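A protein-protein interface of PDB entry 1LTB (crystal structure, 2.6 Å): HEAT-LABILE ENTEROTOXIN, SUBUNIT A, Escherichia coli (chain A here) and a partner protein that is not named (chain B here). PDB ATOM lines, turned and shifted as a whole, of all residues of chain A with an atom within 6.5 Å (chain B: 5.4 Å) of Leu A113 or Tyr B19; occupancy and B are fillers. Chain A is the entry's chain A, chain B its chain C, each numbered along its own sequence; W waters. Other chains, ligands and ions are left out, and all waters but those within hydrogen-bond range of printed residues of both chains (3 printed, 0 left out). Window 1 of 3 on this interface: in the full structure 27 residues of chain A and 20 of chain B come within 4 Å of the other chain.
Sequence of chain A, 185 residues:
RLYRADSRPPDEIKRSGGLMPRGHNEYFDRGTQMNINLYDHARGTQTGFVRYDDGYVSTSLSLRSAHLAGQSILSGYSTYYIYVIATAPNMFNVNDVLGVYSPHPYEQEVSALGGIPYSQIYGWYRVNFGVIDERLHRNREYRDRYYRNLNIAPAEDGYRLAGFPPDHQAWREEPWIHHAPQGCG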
ATOM      1  N   PRO A  21      19.755  -1.076  -5.058  1.00  0.00           N
ATOM      2  CA  PRO A  21      19.321  -1.079  -3.677  1.00  0.00           C
ATOM      3  C   PRO A  21      19.146   0.348  -3.186  1.00  0.00           C
ATOM      4  O   PRO A  21      19.569   1.299  -3.858  1.00  0.00           O
ATOM      5  CB  PRO A  21      20.407  -1.834  -2.986  1.00  0.00           C
ATOM      6  CG  PRO A  21      20.907  -2.765  -4.057  1.00  0.00           C
ATOM      7  CD  PRO A  21      20.980  -1.832  -5.228  1.00  0.00           C
ATOM      8  N   TYR A  27      25.292   0.986 -10.150  1.00  0.00           N
ATOM      9  CA  TYR A  27      25.783  -0.349  -9.946  1.00  0.00           C
ATOM     10  C   TYR A  27      27.257  -0.540  -9.663  1.00  0.00           C
ATOM     11  O   TYR A  27      27.557  -1.313  -8.769  1.00  0.00           O
ATOM     12  CB  TYR A  27      25.375  -1.167 -11.167  1.00  0.00           C
ATOM     13  CG  TYR A  27      25.518  -2.670 -10.980  1.00  0.00           C
ATOM     14  CD1 TYR A  27      24.869  -3.328  -9.959  1.00  0.00           C
ATOM     15  CD2 TYR A  27      26.328  -3.375 -11.809  1.00  0.00           C
ATOM     16  CE1 TYR A  27      25.028  -4.684  -9.764  1.00  0.00           C
ATOM     17  CE2 TYR A  27      26.501  -4.731 -11.615  1.00  0.00           C
ATOM     18  CZ  TYR A  27      25.852  -5.375 -10.601  1.00  0.00           C
ATOM     19  OH  TYR A  27      26.053  -6.713 -10.403  1.00  0.00           O
ATOM     20  N   MET A  34      28.164  -0.145   1.133  1.00  0.00           N
ATOM     21  CA  MET A  34      26.754  -0.360   1.253  1.00  0.00           C
ATOM     22  C   MET A  34      26.566  -1.417   2.327  1.00  0.00           C
ATOM     23  O   MET A  34      27.353  -2.374   2.328  1.00  0.00           O
ATOM     24  CB  MET A  34      26.346  -0.782  -0.141  1.00  0.00           C
ATOM     25  CG  MET A  34      24.906  -1.184  -0.355  1.00  0.00           C
ATOM     26  SD  MET A  34      24.691  -1.720  -2.063  1.00  0.00           S
ATOM     27  CE  MET A  34      26.155  -2.684  -2.340  1.00  0.00           C
ATOM     28  N   ILE A  36      25.201  -4.677   3.304  1.00  0.00           N
ATOM     29  CA  ILE A  36      24.560  -5.781   2.607  1.00  0.00           C
ATOM     30  C   ILE A  36      24.279  -6.852   3.659  1.00  0.00           C
ATOM     31  O   ILE A  36      25.247  -7.399   4.221  1.00  0.00           O
ATOM     32  CB  ILE A  36      25.503  -6.375   1.520  1.00  0.00           C
ATOM     33  CG1 ILE A  36      26.080  -5.279   0.633  1.00  0.00           C
ATOM     34  CG2 ILE A  36      24.711  -7.414   0.727  1.00  0.00           C
ATOM     35  CD1 ILE A  36      27.311  -5.576  -0.215  1.00  0.00           C
ATOM     36  N   GLY A  55      21.225  -3.738   0.841  1.00  0.00           N
ATOM     37  CA  GLY A  55      22.010  -4.292  -0.233  1.00  0.00           C
ATOM     38  C   GLY A  55      21.341  -5.300  -1.130  1.00  0.00           C
ATOM     39  O   GLY A  55      22.033  -5.902  -1.949  1.00  0.00           O
ATOM     40  N   TYR A  56      20.047  -5.534  -1.068  1.00  0.00           N
ATOM     41  CA  TYR A  56      19.430  -6.466  -1.992  1.00  0.00           C
ATOM     42  C   TYR A  56      18.217  -5.818  -2.637  1.00  0.00           C
ATOM     43  O   TYR A  56      17.659  -4.929  -2.000  1.00  0.00           O
ATOM     44  CB  TYR A  56      18.961  -7.688  -1.288  1.00  0.00           C
ATOM     45  CG  TYR A  56      20.004  -8.608  -0.716  1.00  0.00           C
ATOM     46  CD1 TYR A  56      20.818  -8.274   0.339  1.00  0.00           C
ATOM     47  CD2 TYR A  56      20.103  -9.827  -1.321  1.00  0.00           C
ATOM     48  CE1 TYR A  56      21.746  -9.199   0.769  1.00  0.00           C
ATOM     49  CE2 TYR A  56      21.020 -10.736  -0.894  1.00  0.00           C
ATOM     50  CZ  TYR A  56      21.822 -10.408   0.135  1.00  0.00           C
ATOM     51  OH  TYR A  56      22.717 -11.357   0.500  1.00  0.00           O
ATOM     52  N   VAL A  57      17.778  -6.194  -3.845  1.00  0.00           N
ATOM     53  CA  VAL A  57      16.564  -5.669  -4.425  1.00  0.00           C
ATOM     54  C   VAL A  57      15.618  -6.832  -4.542  1.00  0.00           C
ATOM     55  O   VAL A  57      16.059  -7.862  -5.021  1.00  0.00           O
ATOM     56  CB  VAL A  57      16.921  -5.075  -5.752  1.00  0.00           C
ATOM     57  CG1 VAL A  57      15.704  -4.779  -6.619  1.00  0.00           C
ATOM     58  CG2 VAL A  57      17.625  -3.753  -5.434  1.00  0.00           C
ATOM     59  N   PRO A  89      23.185 -16.152 -10.872  1.00  0.00           N
ATOM     60  CA  PRO A  89      23.650 -16.440  -9.519  1.00  0.00           C
ATOM     61  C   PRO A  89      23.658 -15.241  -8.577  1.00  0.00           C
ATOM     62  O   PRO A  89      23.976 -15.421  -7.417  1.00  0.00           O
ATOM     63  CB  PRO A  89      25.027 -17.049  -9.713  1.00  0.00           C
ATOM     64  CG  PRO A  89      24.878 -17.743 -11.035  1.00  0.00           C
ATOM     65  CD  PRO A  89      24.130 -16.669 -11.844  1.00  0.00           C
ATOM     66  N   ASN A  90      23.336 -14.002  -8.931  1.00  0.00           N
ATOM     67  CA  ASN A  90      23.306 -12.915  -7.954  1.00  0.00           C
ATOM     68  C   ASN A  90      21.940 -12.965  -7.249  1.00  0.00           C
ATOM     69  O   ASN A  90      21.642 -12.191  -6.336  1.00  0.00           O
ATOM     70  CB  ASN A  90      23.477 -11.508  -8.610  1.00  0.00           C
ATOM     71  CG  ASN A  90      22.452 -11.157  -9.710  1.00  0.00           C
ATOM     72  OD1 ASN A  90      21.823 -12.032 -10.338  1.00  0.00           O
ATOM     73  ND2 ASN A  90      22.245  -9.895 -10.047  1.00  0.00           N
ATOM     74  N   MET A  91      21.059 -13.880  -7.622  1.00  0.00           N
ATOM     75  CA  MET A  91      19.743 -13.910  -7.065  1.00  0.00           C
ATOM     76  C   MET A  91      19.787 -15.021  -6.028  1.00  0.00           C
ATOM     77  O   MET A  91      20.411 -16.065  -6.274  1.00  0.00           O
ATOM     78  CB  MET A  91      18.671 -14.246  -8.147  1.00  0.00           C
ATOM     79  CG  MET A  91      18.322 -13.347  -9.359  1.00  0.00           C
ATOM     80  SD  MET A  91      18.021 -11.569  -9.100  1.00  0.00           S
ATOM     81  CE  MET A  91      16.635 -11.431  -8.029  1.00  0.00           C
ATOM     82  N   PHE A  92      19.104 -14.826  -4.887  1.00  0.00           N
ATOM     83  CA  PHE A  92      18.941 -15.808  -3.826  1.00  0.00           C
ATOM     84  C   PHE A  92      17.480 -16.043  -3.510  1.00  0.00           C
ATOM     85  O   PHE A  92      16.709 -15.084  -3.365  1.00  0.00           O
ATOM     86  CB  PHE A  92      19.601 -15.335  -2.571  1.00  0.00           C
ATOM     87  CG  PHE A  92      21.094 -15.465  -2.690  1.00  0.00           C
ATOM     88  CD1 PHE A  92      21.688 -16.707  -2.597  1.00  0.00           C
ATOM     89  CD2 PHE A  92      21.846 -14.341  -2.891  1.00  0.00           C
ATOM     90  CE1 PHE A  92      23.053 -16.813  -2.712  1.00  0.00           C
ATOM     91  CE2 PHE A  92      23.210 -14.470  -3.004  1.00  0.00           C
ATOM     92  CZ  PHE A  92      23.818 -15.697  -2.919  1.00  0.00           C
ATOM     93  N   SER A 111      15.815 -12.428  -3.916  1.00  0.00           N
ATOM     94  CA  SER A 111      16.561 -11.181  -3.844  1.00  0.00           C
ATOM     95  C   SER A 111      17.850 -11.145  -4.622  1.00  0.00           C
ATOM     96  O   SER A 111      18.540 -12.159  -4.717  1.00  0.00           O
ATOM     97  CB  SER A 111      16.873 -10.873  -2.410  1.00  0.00           C
ATOM     98  OG  SER A 111      15.667 -10.396  -1.810  1.00  0.00           O
ATOM     99  N   ALA A 112      18.215 -10.014  -5.209  1.00  0.00           N
ATOM    100  CA  ALA A 112      19.463  -9.941  -5.923  1.00  0.00           C
ATOM    101  C   ALA A 112      20.400  -9.171  -5.066  1.00  0.00           C
ATOM    102  O   ALA A 112      20.090  -8.065  -4.613  1.00  0.00           O
ATOM    103  CB  ALA A 112      19.344  -9.193  -7.215  1.00  0.00           C
ATOM    104  N   LEU A 113      21.545  -9.784  -4.828  1.00  0.00           N
ATOM    105  CA  LEU A 113      22.603  -9.168  -4.068  1.00  0.00           C
ATOM    106  C   LEU A 113      23.252  -8.115  -4.956  1.00  0.00           C
ATOM    107  O   LEU A 113      23.725  -8.474  -6.027  1.00  0.00           O
ATOM    108  CB  LEU A 113      23.552 -10.310  -3.662  1.00  0.00           C
ATOM    109  CG  LEU A 113      24.991 -10.187  -3.095  1.00  0.00           C
ATOM    110  CD1 LEU A 113      25.302  -8.881  -2.427  1.00  0.00           C
ATOM    111  CD2 LEU A 113      25.126 -11.324  -2.138  1.00  0.00           C
ATOM    112  N   GLY A 114      23.198  -6.845  -4.527  1.00  0.00           N
ATOM    113  CA  GLY A 114      23.877  -5.749  -5.177  1.00  0.00           C
ATOM    114  C   GLY A 114      23.108  -4.949  -6.199  1.00  0.00           C
ATOM    115  O   GLY A 114      23.616  -3.963  -6.758  1.00  0.00           O
ATOM    116  N   GLY A 115      21.869  -5.346  -6.439  1.00  0.00           N
ATOM    117  CA  GLY A 115      21.045  -4.661  -7.416  1.00  0.00           C
ATOM    118  C   GLY A 115      20.921  -5.542  -8.624  1.00  0.00           C
ATOM    119  O   GLY A 115      21.610  -6.563  -8.619  1.00  0.00           O
ATOM    120  N   ILE A 116      20.071  -5.259  -9.623  1.00  0.00           N
ATOM    121  CA  ILE A 116      19.960  -6.090 -10.824  1.00  0.00           C
ATOM    122  C   ILE A 116      20.650  -5.252 -11.860  1.00  0.00           C
ATOM    123  O   ILE A 116      20.163  -4.126 -12.043  1.00  0.00           O
ATOM    124  CB  ILE A 116      18.490  -6.329 -11.276  1.00  0.00           C
ATOM    125  CG1 ILE A 116      17.731  -7.308 -10.394  1.00  0.00           C
ATOM    126  CG2 ILE A 116      18.494  -7.045 -12.603  1.00  0.00           C
ATOM    127  CD1 ILE A 116      16.950  -6.762  -9.187  1.00  0.00           C
ATOM    128  N   ALA A 153      21.190 -18.589  -7.499  1.00  0.00           N
ATOM    129  CA  ALA A 153      22.270 -19.170  -6.756  1.00  0.00           C
ATOM    130  C   ALA A 153      21.650 -20.174  -5.828  1.00  0.00           C
ATOM    131  O   ALA A 153      20.535 -19.917  -5.360  1.00  0.00           O
ATOM    132  CB  ALA A 153      22.962 -18.140  -5.946  1.00  0.00           C
ATOM    133  N   PRO A 154      22.281 -21.325  -5.541  1.00  0.00           N
ATOM    134  CA  PRO A 154      21.767 -22.352  -4.623  1.00  0.00           C
ATOM    135  C   PRO A 154      21.797 -21.861  -3.158  1.00  0.00           C
ATOM    136  O   PRO A 154      22.735 -21.120  -2.788  1.00  0.00           O
ATOM    137  CB  PRO A 154      22.669 -23.548  -4.907  1.00  0.00           C
ATOM    138  CG  PRO A 154      23.242 -23.296  -6.290  1.00  0.00           C
ATOM    139  CD  PRO A 154      23.504 -21.804  -6.183  1.00  0.00           C
ATOM    140  N   ASP A 157      25.076 -21.683  -1.115  1.00  0.00           N
ATOM    141  CA  ASP A 157      25.951 -20.538  -1.269  1.00  0.00           C
ATOM    142  C   ASP A 157      25.436 -19.339  -0.491  1.00  0.00           C
ATOM    143  O   ASP A 157      26.158 -18.395  -0.148  1.00  0.00           O
ATOM    144  CB  ASP A 157      26.043 -20.235  -2.742  1.00  0.00           C
ATOM    145  CG  ASP A 157      26.736 -21.299  -3.587  1.00  0.00           C
ATOM    146  OD1 ASP A 157      27.372 -22.212  -3.062  1.00  0.00           O
ATOM    147  OD2 ASP A 157      26.658 -21.201  -4.807  1.00  0.00           O
ATOM    148  N   GLY A 158      24.136 -19.406  -0.209  1.00  0.00           N
ATOM    149  CA  GLY A 158      23.456 -18.356   0.506  1.00  0.00           C
ATOM    150  C   GLY A 158      23.626 -18.497   1.980  1.00  0.00           C
ATOM    151  O   GLY A 158      23.712 -17.469   2.645  1.00  0.00           O
ATOM    152  N   ARG A 160      25.993 -19.004   4.260  1.00  0.00           N
ATOM    153  CA  ARG A 160      26.994 -18.211   4.954  1.00  0.00           C
ATOM    154  C   ARG A 160      26.644 -16.741   4.856  1.00  0.00           C
ATOM    155  O   ARG A 160      27.222 -15.935   5.582  1.00  0.00           O
ATOM    156  CB  ARG A 160      28.383 -18.395   4.359  1.00  0.00           C
ATOM    157  CG  ARG A 160      28.268 -18.107   2.868  1.00  0.00           C
ATOM    158  CD  ARG A 160      29.467 -18.357   1.976  1.00  0.00           C
ATOM    159  NE  ARG A 160      29.037 -18.575   0.587  1.00  0.00           N
ATOM    160  CZ  ARG A 160      29.385 -17.786  -0.447  1.00  0.00           C
ATOM    161  NH1 ARG A 160      30.172 -16.705  -0.282  1.00  0.00           N
ATOM    162  NH2 ARG A 160      28.944 -18.115  -1.668  1.00  0.00           N
ATOM    163  N   LEU A 161      25.737 -16.389   3.937  1.00  0.00           N
ATOM    164  CA  LEU A 161      25.383 -14.999   3.694  1.00  0.00           C
ATOM    165  C   LEU A 161      24.100 -14.473   4.298  1.00  0.00           C
ATOM    166  O   LEU A 161      23.783 -13.278   4.165  1.00  0.00           O
ATOM    167  CB  LEU A 161      25.355 -14.774   2.192  1.00  0.00           C
ATOM    168  CG  LEU A 161      26.689 -14.839   1.441  1.00  0.00           C
ATOM    169  CD1 LEU A 161      26.434 -14.731  -0.067  1.00  0.00           C
ATOM    170  CD2 LEU A 161      27.615 -13.733   1.957  1.00  0.00           C
ATOM    171  N   ASN B  14      31.680  -8.479   4.430  1.00  0.00           N
ATOM    172  CA  ASN B  14      32.916  -8.796   3.760  1.00  0.00           C
ATOM    173  C   ASN B  14      32.690 -10.025   2.883  1.00  0.00           C
ATOM    174  O   ASN B  14      33.134 -10.008   1.740  1.00  0.00           O
ATOM    175  CB  ASN B  14      33.893  -8.948   4.932  1.00  0.00           C
ATOM    176  CG  ASN B  14      35.217  -9.651   4.708  1.00  0.00           C
ATOM    177  OD1 ASN B  14      36.135  -9.083   4.122  1.00  0.00           O
ATOM    178  ND2 ASN B  14      35.448 -10.868   5.199  1.00  0.00           N
ATOM    179  N   LEU B  15      31.974 -11.092   3.258  1.00  0.00           N
ATOM    180  CA  LEU B  15      31.772 -12.236   2.369  1.00  0.00           C
ATOM    181  C   LEU B  15      30.778 -11.881   1.287  1.00  0.00           C
ATOM    182  O   LEU B  15      30.916 -12.357   0.154  1.00  0.00           O
ATOM    183  CB  LEU B  15      31.218 -13.427   3.092  1.00  0.00           C
ATOM    184  CG  LEU B  15      31.988 -13.928   4.310  1.00  0.00           C
ATOM    185  CD1 LEU B  15      31.072 -14.848   5.102  1.00  0.00           C
ATOM    186  CD2 LEU B  15      33.301 -14.564   3.886  1.00  0.00           C
ATOM    187  N   SER B  16      29.780 -11.048   1.666  1.00  0.00           N
ATOM    188  CA  SER B  16      28.764 -10.521   0.790  1.00  0.00           C
ATOM    189  C   SER B  16      29.350  -9.668  -0.300  1.00  0.00           C
ATOM    190  O   SER B  16      29.136  -9.989  -1.459  1.00  0.00           O
ATOM    191  CB  SER B  16      27.788  -9.738   1.628  1.00  0.00           C
ATOM    192  OG  SER B  16      26.997 -10.681   2.332  1.00  0.00           O
ATOM    193  N   THR B  17      30.104  -8.612   0.034  1.00  0.00           N
ATOM    194  CA  THR B  17      30.856  -7.837  -0.927  1.00  0.00           C
ATOM    195  C   THR B  17      31.806  -8.718  -1.759  1.00  0.00           C
ATOM    196  O   THR B  17      31.931  -8.452  -2.960  1.00  0.00           O
ATOM    197  CB  THR B  17      31.663  -6.732  -0.184  1.00  0.00           C
ATOM    198  OG1 THR B  17      30.700  -5.816   0.373  1.00  0.00           O
ATOM    199  CG2 THR B  17      32.608  -5.961  -1.082  1.00  0.00           C
ATOM    200  N   ILE B  18      32.505  -9.751  -1.272  1.00  0.00           N
ATOM    201  CA  ILE B  18      33.329 -10.511  -2.175  1.00  0.00           C
ATOM    202  C   ILE B  18      32.379 -11.189  -3.128  1.00  0.00           C
ATOM    203  O   ILE B  18      32.629 -11.086  -4.301  1.00  0.00           O
ATOM    204  CB  ILE B  18      34.150 -11.505  -1.408  1.00  0.00           C
ATOM    205  CG1 ILE B  18      35.216 -10.705  -0.665  1.00  0.00           C
ATOM    206  CG2 ILE B  18      34.717 -12.564  -2.330  1.00  0.00           C
ATOM    207  CD1 ILE B  18      36.318 -11.587  -0.055  1.00  0.00           C
ATOM    208  N   TYR B  19      31.248 -11.740  -2.739  1.00  0.00           N
ATOM    209  CA  TYR B  19      30.279 -12.273  -3.658  1.00  0.00           C
ATOM    210  C   TYR B  19      29.786 -11.167  -4.604  1.00  0.00           C
ATOM    211  O   TYR B  19      29.611 -11.444  -5.791  1.00  0.00           O
ATOM    212  CB  TYR B  19      29.113 -12.863  -2.863  1.00  0.00           C
ATOM    213  CG  TYR B  19      28.243 -13.785  -3.696  1.00  0.00           C
ATOM    214  CD1 TYR B  19      27.341 -13.306  -4.660  1.00  0.00           C
ATOM    215  CD2 TYR B  19      28.422 -15.119  -3.525  1.00  0.00           C
ATOM    216  CE1 TYR B  19      26.652 -14.178  -5.473  1.00  0.00           C
ATOM    217  CE2 TYR B  19      27.726 -15.986  -4.335  1.00  0.00           C
ATOM    218  CZ  TYR B  19      26.854 -15.506  -5.283  1.00  0.00           C
ATOM    219  OH  TYR B  19      26.196 -16.418  -6.049  1.00  0.00           O
ATOM    220  N   LEU B  20      29.532  -9.924  -4.256  1.00  0.00           N
ATOM    221  CA  LEU B  20      29.142  -8.941  -5.251  1.00  0.00           C
ATOM    222  C   LEU B  20      30.243  -8.560  -6.254  1.00  0.00           C
ATOM    223  O   LEU B  20      29.943  -8.383  -7.436  1.00  0.00           O
ATOM    224  CB  LEU B  20      28.664  -7.673  -4.559  1.00  0.00           C
ATOM    225  CG  LEU B  20      28.102  -6.588  -5.497  1.00  0.00           C
ATOM    226  CD1 LEU B  20      26.922  -7.107  -6.377  1.00  0.00           C
ATOM    227  CD2 LEU B  20      27.719  -5.431  -4.624  1.00  0.00           C
ATOM    228  N   ARG B  21      31.518  -8.427  -5.847  1.00  0.00           N
ATOM    229  CA  ARG B  21      32.603  -7.923  -6.688  1.00  0.00           C
ATOM    230  C   ARG B  21      32.968  -8.895  -7.784  1.00  0.00           C
ATOM    231  O   ARG B  21      33.270  -8.559  -8.935  1.00  0.00           O
ATOM    232  CB  ARG B  21      33.832  -7.629  -5.841  1.00  0.00           C
ATOM    233  CG  ARG B  21      33.478  -6.563  -4.828  1.00  0.00           C
ATOM    234  CD  ARG B  21      33.848  -5.113  -5.120  1.00  0.00           C
ATOM    235  NE  ARG B  21      32.749  -4.221  -4.723  1.00  0.00           N
ATOM    236  CZ  ARG B  21      32.851  -3.152  -3.898  1.00  0.00           C
ATOM    237  NH1 ARG B  21      34.016  -2.773  -3.308  1.00  0.00           N
ATOM    238  NH2 ARG B  21      31.743  -2.394  -3.724  1.00  0.00           N
ATOM    239  N   GLU B  22      32.838 -10.139  -7.426  1.00  0.00           N
ATOM    240  CA  GLU B  22      33.073 -11.216  -8.356  1.00  0.00           C
ATOM    241  C   GLU B  22      32.019 -11.131  -9.441  1.00  0.00           C
ATOM    242  O   GLU B  22      32.393 -11.069 -10.620  1.00  0.00           O
ATOM    243  CB  GLU B  22      32.969 -12.577  -7.676  1.00  0.00           C
ATOM    244  CG  GLU B  22      33.842 -12.629  -6.416  1.00  0.00           C
ATOM    245  CD  GLU B  22      35.086 -13.502  -6.439  1.00  0.00           C
ATOM    246  OE1 GLU B  22      34.934 -14.724  -6.624  1.00  0.00           O
ATOM    247  OE2 GLU B  22      36.184 -12.946  -6.251  1.00  0.00           O
ATOM    248  N   TYR B  23      30.730 -11.025  -9.040  1.00  0.00           N
ATOM    249  CA  TYR B  23      29.634 -10.923  -9.982  1.00  0.00           C
ATOM    250  C   TYR B  23      29.845  -9.676 -10.815  1.00  0.00           C
ATOM    251  O   TYR B  23      29.796  -9.828 -12.017  1.00  0.00           O
ATOM    252  CB  TYR B  23      28.276 -10.859  -9.267  1.00  0.00           C
ATOM    253  CG  TYR B  23      27.154 -11.055 -10.301  1.00  0.00           C
ATOM    254  CD1 TYR B  23      26.927 -12.278 -10.916  1.00  0.00           C
ATOM    255  CD2 TYR B  23      26.326  -9.998 -10.618  1.00  0.00           C
ATOM    256  CE1 TYR B  23      25.906 -12.429 -11.835  1.00  0.00           C
ATOM    257  CE2 TYR B  23      25.308 -10.147 -11.523  1.00  0.00           C
ATOM    258  CZ  TYR B  23      25.113 -11.351 -12.132  1.00  0.00           C
ATOM    259  OH  TYR B  23      24.119 -11.441 -13.098  1.00  0.00           O
HETATM  260  O   HOH W   1      23.872 -10.775   3.015  1.00  0.00           O
HETATM  261  O   HOH W   2      29.659  -3.313   1.337  1.00  0.00           O
HETATM  262  O   HOH W   3      32.282 -15.076  -1.329  1.00  0.00           O
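Water W2 bridges the backbone carbonyl oxygen of Met A34 and the side-chain hydroxyl of Thr B17.
Water W1 lies within hydrogen-bond range of the backbone carbonyl oxygen (O) of Leu A161 (2.8 Å), the side-chain hydroxyl (OH) of Tyr A56 (2.8 Å) and the side-chain hydroxyl (OG) of Ser B16 (3.2 Å).
Water W3 lies within hydrogen-bond range of NH1 of Arg A160 (2.9 Å) and O of Leu B15 (3.4 Å).
The backbone carbonyl oxygen (O) of Pro A89 sits at hydrogen-bond distance from the side-chain hydroxyl (OH) of Tyr B19, at 2.8 Å.
Among the printed residues, pairs that only touch across the chains: Tyr A27 with Tyr B23 (3.3 Å), Met A34 with Leu B20 (3.9 Å), Ile A36 with Ser B16 (3.96 Å), Ile A36 with Thr B17 (3.4 Å), Asn A90 with Tyr B23 (3.4 Å), Phe A92 with Tyr B19 (3.9 Å), Leu A113 with Tyr B19 (3.9 Å), Leu A113 with Leu B20 (3.5 Å), Gly A114 with Leu B20 (3.5 Å), Ala A153 with Tyr B19 (3.7 Å), Arg A160 with Tyr B19 (3.6 Å), Leu A161 with Leu B15 (3.7 Å) and Leu A161 with Ser B16 (3.1 Å).
The backbone NH (N) of Gly A114 is in hydrogen-bond range of the backbone carbonyl oxygen (O) of Gly A55 (3.0 Å).
The backbone NH (N) of Leu A113 sits at hydrogen-bond distance from the backbone carbonyl oxygen (O) of Asn A90 (2.8 Å).
The backbone carbonyl oxygen of Met A91 sits at hydrogen-bond distance from the backbone NH of Ala A153.
The backbone carbonyl oxygen of Ser A111 is in hydrogen-bond range of the backbone NH of Phe A92, at 2.7 Å.
O of Asp A157 is in hydrogen-bond range of NE of Arg A160 (3.0 Å).
Of the 23 printed residues of chain A, 11 touch a printed residue of chain B.
Hydrophobic or aromatic side chains of chain A within 4 Å of the printed part of chain B: Tyr A27, Met A34, Ile A36, Pro A89, Phe A92, Leu A113, Ala A153 and Leu A161.
Of the 10 printed residues of chain B, 6 touch a printed residue of chain A.
Printed residues of chain B that touch a printed residue of chain A: Leu B15, Ser B16, Thr B17, Tyr B19, Leu B20 and Tyr B23.
Hydrophobic or aromatic side chains of chain B within 4 Å of the printed part of chain A: Leu B15, Tyr B19, Leu B20 and Tyr B23.
Along chain B the printed residues that touch a printed residue of chain A span positions 15 to 23.
Among the printed residues, no Asp or Glu carboxylate lies within 4 Å of a Lys or Arg side-chain nitrogen of the other chain.
Of the printed residues of chain B, Pro A89 touches Tyr B19 (2.8 Å).
Leu A113 touches two residues of chain B.
Printed residues of chain B within 4 Å of Gly A114: Leu B20.
Of the printed residues of chain A, Ser B16 touches Ile A36 and Leu A161.
Of the printed residues of chain A, Thr B17 touches Ile A36 (3.4 Å).
Printed residues of chain A within 4 Å of Tyr B19: Pro A89 (2.8 Å), Phe A92 (3.9 Å), Leu A113 (3.9 Å), Ala A153 (3.7 Å) and Arg A160 (3.6 Å).
Printed residues of chain A within 4 Å of Tyr B23: Tyr A27 and Asn A90.
The nearest printed residue of chain A that does not touch Tyr B19 is Leu A161 (4.01 Å).
The nearest printed residue of chain B that does not touch Pro A89 is Tyr B23 (4.6 Å).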
